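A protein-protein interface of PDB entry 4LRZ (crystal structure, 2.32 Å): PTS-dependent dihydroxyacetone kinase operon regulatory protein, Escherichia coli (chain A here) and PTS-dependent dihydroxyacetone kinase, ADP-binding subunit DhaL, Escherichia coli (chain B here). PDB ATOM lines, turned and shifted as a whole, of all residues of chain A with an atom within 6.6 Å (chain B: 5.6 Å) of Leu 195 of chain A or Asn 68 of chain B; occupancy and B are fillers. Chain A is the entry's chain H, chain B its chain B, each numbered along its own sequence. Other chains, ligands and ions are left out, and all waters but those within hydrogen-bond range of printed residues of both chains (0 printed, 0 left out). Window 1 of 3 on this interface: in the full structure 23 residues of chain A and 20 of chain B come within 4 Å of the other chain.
Printed residues of chain B within 4 Å of Leu 195 of chain A: Phe 64 (3.97 Å), Asn 68 (3.7 Å) and Met 71 (3.5 Å).
Ala 196 of chain A touches none of the printed residues of chain B.
Printed residues of chain B within 4 Å of Thr 198 of chain A: Phe 64.
Of the printed residues of chain B, Asn 199 of chain A touches Ile 57 (3.5 Å) and Phe 64 (3.7 Å).
Printed residues of chain A within 4 Å of Asn 68 of chain B: Leu 195.
Printed residues of chain A within 4 Å of Met 71 of chain B: Leu 195 (3.5 Å).
The nearest residue of chain A that does not touch Asn 68 of chain B is Ala 196 of chain A (5.6 Å).
Among the printed residues, pairs that only touch across the chains: Asn 199 of chain A with Ile 57 of chain B (3.5 Å), Leu 195 of chain A with Met 71 of chain B (3.5 Å), Leu 195 of chain A with Asn 68 of chain B (3.7 Å), Asn 199 of chain A with Phe 64 of chain B (3.7 Å), Thr 198 of chain A with Phe 64 of chain B (3.9 Å) and Leu 195 of chain A with Phe 64 of chain B (3.97 Å).
The backbone carbonyl oxygen of Phe 64 of chain B lies close to the side-chain amide oxygen of Asn 68 of chain B.
O of Asn 68 of chain B lies within hydrogen-bond range of OG1 of Thr 72 of chain B (3.2 Å).
Hydrophobic or aromatic side chains of chain A within 4 Å of the printed part of chain B: Leu 195.
Of the 12 printed residues of chain B, 4 touch a printed residue of chain A.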
ATOM      1  N   LEU A 190       5.254  18.607 -18.596  1.00  0.00           N
ATOM      2  CA  LEU A 190       4.743  17.521 -17.815  1.00  0.00           C
ATOM      3  C   LEU A 190       4.756  16.207 -18.600  1.00  0.00           C
ATOM      4  O   LEU A 190       5.083  15.167 -18.038  1.00  0.00           O
ATOM      5  CB  LEU A 190       3.335  17.863 -17.330  1.00  0.00           C
ATOM      6  CG  LEU A 190       2.639  16.804 -16.486  1.00  0.00           C
ATOM      7  CD1 LEU A 190       3.400  16.731 -15.161  1.00  0.00           C
ATOM      8  CD2 LEU A 190       1.155  17.142 -16.265  1.00  0.00           C
ATOM      9  N   THR A 191       4.402  16.250 -19.882  1.00  0.00           N
ATOM     10  CA  THR A 191       4.345  15.027 -20.668  1.00  0.00           C
ATOM     11  C   THR A 191       5.760  14.549 -20.923  1.00  0.00           C
ATOM     12  O   THR A 191       6.001  13.356 -20.915  1.00  0.00           O
ATOM     13  CB  THR A 191       3.536  15.133 -21.998  1.00  0.00           C
ATOM     14  OG1 THR A 191       4.353  15.646 -23.058  1.00  0.00           O
ATOM     15  CG2 THR A 191       2.391  16.039 -21.841  1.00  0.00           C
ATOM     16  N   ASP A 192       6.706  15.467 -21.102  1.00  0.00           N
ATOM     17  CA  ASP A 192       8.113  15.033 -21.137  1.00  0.00           C
ATOM     18  C   ASP A 192       8.486  14.260 -19.890  1.00  0.00           C
ATOM     19  O   ASP A 192       9.197  13.249 -19.949  1.00  0.00           O
ATOM     20  CB  ASP A 192       9.117  16.183 -21.388  1.00  0.00           C
ATOM     21  CG  ASP A 192       9.225  16.568 -22.904  1.00  0.00           C
ATOM     22  OD1 ASP A 192       9.064  15.669 -23.775  1.00  0.00           O
ATOM     23  OD2 ASP A 192       9.458  17.756 -23.236  1.00  0.00           O
ATOM     24  N   SER A 193       8.007  14.707 -18.747  1.00  0.00           N
ATOM     25  CA  SER A 193       8.424  14.039 -17.519  1.00  0.00           C
ATOM     26  C   SER A 193       7.696  12.696 -17.267  1.00  0.00           C
ATOM     27  O   SER A 193       8.295  11.767 -16.766  1.00  0.00           O
ATOM     28  CB  SER A 193       8.496  15.006 -16.329  1.00  0.00           C
ATOM     29  OG  SER A 193       7.406  14.895 -15.446  1.00  0.00           O
ATOM     30  N   LEU A 194       6.454  12.563 -17.750  1.00  0.00           N
ATOM     31  CA  LEU A 194       5.707  11.273 -17.653  1.00  0.00           C
ATOM     32  C   LEU A 194       6.371  10.196 -18.442  1.00  0.00           C
ATOM     33  O   LEU A 194       6.513   9.095 -17.962  1.00  0.00           O
ATOM     34  CB  LEU A 194       4.239  11.424 -18.080  1.00  0.00           C
ATOM     35  CG  LEU A 194       3.475  12.422 -17.230  1.00  0.00           C
ATOM     36  CD1 LEU A 194       2.149  12.862 -17.878  1.00  0.00           C
ATOM     37  CD2 LEU A 194       3.322  11.885 -15.787  1.00  0.00           C
ATOM     38  N   LEU A 195       6.776  10.509 -19.668  1.00  0.00           N
ATOM     39  CA  LEU A 195       7.575   9.603 -20.504  1.00  0.00           C
ATOM     40  C   LEU A 195       8.893   9.146 -19.852  1.00  0.00           C
ATOM     41  O   LEU A 195       9.245   7.976 -19.930  1.00  0.00           O
ATOM     42  CB  LEU A 195       7.902  10.312 -21.821  1.00  0.00           C
ATOM     43  CG  LEU A 195       6.830  10.403 -22.907  1.00  0.00           C
ATOM     44  CD1 LEU A 195       7.206  11.507 -23.907  1.00  0.00           C
ATOM     45  CD2 LEU A 195       6.660   9.020 -23.600  1.00  0.00           C
ATOM     46  N   ALA A 196       9.631  10.063 -19.236  1.00  0.00           N
ATOM     47  CA  ALA A 196      10.802   9.691 -18.417  1.00  0.00           C
ATOM     48  C   ALA A 196      10.416   8.738 -17.279  1.00  0.00           C
ATOM     49  O   ALA A 196      11.078   7.681 -17.070  1.00  0.00           O
ATOM     50  CB  ALA A 196      11.523  10.936 -17.848  1.00  0.00           C
ATOM     51  N   GLU A 197       9.347   9.074 -16.555  1.00  0.00           N
ATOM     52  CA  GLU A 197       8.881   8.182 -15.472  1.00  0.00           C
ATOM     53  C   GLU A 197       8.526   6.798 -16.018  1.00  0.00           C
ATOM     54  O   GLU A 197       8.956   5.778 -15.485  1.00  0.00           O
ATOM     55  CB  GLU A 197       7.734   8.824 -14.656  1.00  0.00           C
ATOM     56  CG  GLU A 197       8.199  10.197 -14.008  1.00  0.00           C
ATOM     57  CD  GLU A 197       7.335  10.749 -12.833  1.00  0.00           C
ATOM     58  OE1 GLU A 197       6.825  11.899 -12.950  1.00  0.00           O
ATOM     59  OE2 GLU A 197       7.206  10.053 -11.783  1.00  0.00           O
ATOM     60  N   THR A 198       7.779   6.743 -17.118  1.00  0.00           N
ATOM     61  CA  THR A 198       7.540   5.449 -17.702  1.00  0.00           C
ATOM     62  C   THR A 198       8.807   4.723 -18.157  1.00  0.00           C
ATOM     63  O   THR A 198       8.936   3.540 -17.919  1.00  0.00           O
ATOM     64  CB  THR A 198       6.383   5.394 -18.741  1.00  0.00           C
ATOM     65  OG1 THR A 198       6.651   4.364 -19.715  1.00  0.00           O
ATOM     66  CG2 THR A 198       6.255   6.595 -19.406  1.00  0.00           C
ATOM     67  N   ASN A 199       9.773   5.434 -18.723  1.00  0.00           N
ATOM     68  CA  ASN A 199      11.082   4.850 -19.030  1.00  0.00           C
ATOM     69  C   ASN A 199      11.748   4.238 -17.784  1.00  0.00           C
ATOM     70  O   ASN A 199      12.297   3.150 -17.836  1.00  0.00           O
ATOM     71  CB  ASN A 199      11.993   5.940 -19.686  1.00  0.00           C
ATOM     72  CG  ASN A 199      13.304   5.371 -20.253  1.00  0.00           C
ATOM     73  OD1 ASN A 199      13.306   4.420 -21.036  1.00  0.00           O
ATOM     74  ND2 ASN A 199      14.418   5.969 -19.863  1.00  0.00           N
ATOM     75  N   ARG A 200      11.695   4.927 -16.651  1.00  0.00           N
ATOM     76  CA  ARG A 200      12.297   4.403 -15.423  1.00  0.00           C
ATOM     77  C   ARG A 200      11.635   3.109 -14.931  1.00  0.00           C
ATOM     78  O   ARG A 200      12.297   2.198 -14.393  1.00  0.00           O
ATOM     79  CB  ARG A 200      12.351   5.482 -14.351  1.00  0.00           C
ATOM     80  CG  ARG A 200      13.217   6.666 -14.806  1.00  0.00           C
ATOM     81  CD  ARG A 200      13.787   7.488 -13.624  1.00  0.00           C
ATOM     82  NE  ARG A 200      14.732   6.697 -12.835  1.00  0.00           N
ATOM     83  CZ  ARG A 200      15.087   6.986 -11.583  1.00  0.00           C
ATOM     84  NH1 ARG A 200      14.587   8.060 -10.991  1.00  0.00           N
ATOM     85  NH2 ARG A 200      15.926   6.197 -10.926  1.00  0.00           N
ATOM     86  N   ILE B  57      16.574   5.857 -23.916  1.00  0.00           N
ATOM     87  CA  ILE B  57      15.561   4.917 -24.449  1.00  0.00           C
ATOM     88  C   ILE B  57      16.083   3.884 -25.476  1.00  0.00           C
ATOM     89  O   ILE B  57      15.326   3.025 -25.970  1.00  0.00           O
ATOM     90  CB  ILE B  57      14.289   5.658 -24.984  1.00  0.00           C
ATOM     91  CG1 ILE B  57      14.627   6.542 -26.184  1.00  0.00           C
ATOM     92  CG2 ILE B  57      13.621   6.521 -23.857  1.00  0.00           C
ATOM     93  CD1 ILE B  57      13.438   7.269 -26.778  1.00  0.00           C
ATOM     94  N   GLY B  63       8.623   0.545 -30.699  1.00  0.00           N
ATOM     95  CA  GLY B  63       7.393   1.314 -30.547  1.00  0.00           C
ATOM     96  C   GLY B  63       7.588   2.460 -29.565  1.00  0.00           C
ATOM     97  O   GLY B  63       7.223   3.598 -29.851  1.00  0.00           O
ATOM     98  N   PHE B  64       8.187   2.183 -28.416  1.00  0.00           N
ATOM     99  CA  PHE B  64       8.491   3.217 -27.411  1.00  0.00           C
ATOM    100  C   PHE B  64       9.450   4.286 -27.933  1.00  0.00           C
ATOM    101  O   PHE B  64       9.238   5.454 -27.701  1.00  0.00           O
ATOM    102  CB  PHE B  64       9.030   2.576 -26.128  1.00  0.00           C
ATOM    103  CG  PHE B  64       9.093   3.508 -24.962  1.00  0.00           C
ATOM    104  CD1 PHE B  64       7.912   4.038 -24.400  1.00  0.00           C
ATOM    105  CD2 PHE B  64      10.312   3.801 -24.372  1.00  0.00           C
ATOM    106  CE1 PHE B  64       7.951   4.868 -23.327  1.00  0.00           C
ATOM    107  CE2 PHE B  64      10.374   4.646 -23.283  1.00  0.00           C
ATOM    108  CZ  PHE B  64       9.187   5.187 -22.758  1.00  0.00           C
ATOM    109  N   ILE B  65      10.472   3.875 -28.674  1.00  0.00           N
ATOM    110  CA  ILE B  65      11.455   4.777 -29.246  1.00  0.00           C
ATOM    111  C   ILE B  65      10.800   5.670 -30.275  1.00  0.00           C
ATOM    112  O   ILE B  65      10.987   6.854 -30.250  1.00  0.00           O
ATOM    113  CB  ILE B  65      12.680   3.973 -29.806  1.00  0.00           C
ATOM    114  CG1 ILE B  65      13.480   3.328 -28.663  1.00  0.00           C
ATOM    115  CG2 ILE B  65      13.603   4.860 -30.669  1.00  0.00           C
ATOM    116  CD1 ILE B  65      14.454   2.242 -29.124  1.00  0.00           C
ATOM    117  N   LEU B  66      10.001   5.120 -31.166  1.00  0.00           N
ATOM    118  CA  LEU B  66       9.297   5.946 -32.185  1.00  0.00           C
ATOM    119  C   LEU B  66       8.218   6.836 -31.549  1.00  0.00           C
ATOM    120  O   LEU B  66       7.956   7.942 -32.011  1.00  0.00           O
ATOM    121  CB  LEU B  66       8.676   5.018 -33.273  1.00  0.00           C
ATOM    122  CG  LEU B  66       9.710   4.216 -34.116  1.00  0.00           C
ATOM    123  CD1 LEU B  66       9.015   3.422 -35.239  1.00  0.00           C
ATOM    124  CD2 LEU B  66      10.903   5.032 -34.710  1.00  0.00           C
ATOM    125  N   LYS B  67       7.637   6.378 -30.450  1.00  0.00           N
ATOM    126  CA  LYS B  67       6.659   7.184 -29.707  1.00  0.00           C
ATOM    127  C   LYS B  67       7.290   8.403 -29.051  1.00  0.00           C
ATOM    128  O   LYS B  67       6.761   9.479 -29.188  1.00  0.00           O
ATOM    129  CB  LYS B  67       5.923   6.355 -28.636  1.00  0.00           C
ATOM    130  CG  LYS B  67       4.825   7.141 -28.012  1.00  0.00           C
ATOM    131  CD  LYS B  67       3.890   6.251 -27.252  1.00  0.00           C
ATOM    132  CE  LYS B  67       4.170   6.331 -25.795  1.00  0.00           C
ATOM    133  NZ  LYS B  67       2.873   6.652 -25.081  1.00  0.00           N
ATOM    134  N   ASN B  68       8.414   8.222 -28.359  1.00  0.00           N
ATOM    135  CA  ASN B  68       9.161   9.348 -27.802  1.00  0.00           C
ATOM    136  C   ASN B  68       9.540  10.338 -28.869  1.00  0.00           C
ATOM    137  O   ASN B  68       9.144  11.482 -28.780  1.00  0.00           O
ATOM    138  CB  ASN B  68      10.368   8.843 -27.055  1.00  0.00           C
ATOM    139  CG  ASN B  68       9.983   8.280 -25.743  1.00  0.00           C
ATOM    140  OD1 ASN B  68       9.443   7.169 -25.643  1.00  0.00           O
ATOM    141  ND2 ASN B  68      10.140   9.088 -24.718  1.00  0.00           N
ATOM    142  N   THR B  69      10.194   9.859 -29.923  1.00  0.00           N
ATOM    143  CA  THR B  69      10.548  10.662 -31.094  1.00  0.00           C
ATOM    144  C   THR B  69       9.379  11.468 -31.680  1.00  0.00           C
ATOM    145  O   THR B  69       9.440  12.704 -31.804  1.00  0.00           O
ATOM    146  CB  THR B  69      11.085   9.713 -32.194  1.00  0.00           C
ATOM    147  OG1 THR B  69      12.179   8.943 -31.663  1.00  0.00           O
ATOM    148  CG2 THR B  69      11.468  10.473 -33.452  1.00  0.00           C
ATOM    149  N   GLY B  70       8.319  10.788 -32.092  1.00  0.00           N
ATOM    150  CA  GLY B  70       7.204  11.534 -32.638  1.00  0.00           C
ATOM    151  C   GLY B  70       6.610  12.539 -31.662  1.00  0.00           C
ATOM    152  O   GLY B  70       6.222  13.646 -32.037  1.00  0.00           O
ATOM    153  N   MET B  71       6.568  12.190 -30.400  1.00  0.00           N
ATOM    154  CA  MET B  71       6.080  13.129 -29.414  1.00  0.00           C
ATOM    155  C   MET B  71       6.935  14.393 -29.286  1.00  0.00           C
ATOM    156  O   MET B  71       6.413  15.496 -29.170  1.00  0.00           O
ATOM    157  CB  MET B  71       6.036  12.454 -28.077  1.00  0.00           C
ATOM    158  CG  MET B  71       4.888  12.919 -27.290  1.00  0.00           C
ATOM    159  SD  MET B  71       3.716  11.557 -27.171  1.00  0.00           S
ATOM    160  CE  MET B  71       4.598  10.426 -26.100  1.00  0.00           C
ATOM    161  N   THR B  72       8.248  14.198 -29.285  1.00  0.00           N
ATOM    162  CA  THR B  72       9.213  15.269 -29.291  1.00  0.00           C
ATOM    163  C   THR B  72       9.069  16.087 -30.569  1.00  0.00           C
ATOM    164  O   THR B  72       8.999  17.297 -30.507  1.00  0.00           O
ATOM    165  CB  THR B  72      10.652  14.706 -29.221  1.00  0.00           C
ATOM    166  OG1 THR B  72      10.845  14.038 -27.970  1.00  0.00           O
ATOM    167  CG2 THR B  72      11.647  15.797 -29.354  1.00  0.00           C
ATOM    168  N   LEU B  73       9.027  15.439 -31.728  1.00  0.00           N
ATOM    169  CA  LEU B  73       8.904  16.209 -32.971  1.00  0.00           C
ATOM    170  C   LEU B  73       7.633  17.009 -32.915  1.00  0.00           C
ATOM    171  O   LEU B  73       7.603  18.179 -33.299  1.00  0.00           O
ATOM    172  CB  LEU B  73       8.902  15.312 -34.210  1.00  0.00           C
ATOM    173  CG  LEU B  73      10.259  14.649 -34.369  1.00  0.00           C
ATOM    174  CD1 LEU B  73      10.234  13.856 -35.610  1.00  0.00           C
ATOM    175  CD2 LEU B  73      11.379  15.670 -34.370  1.00  0.00           C
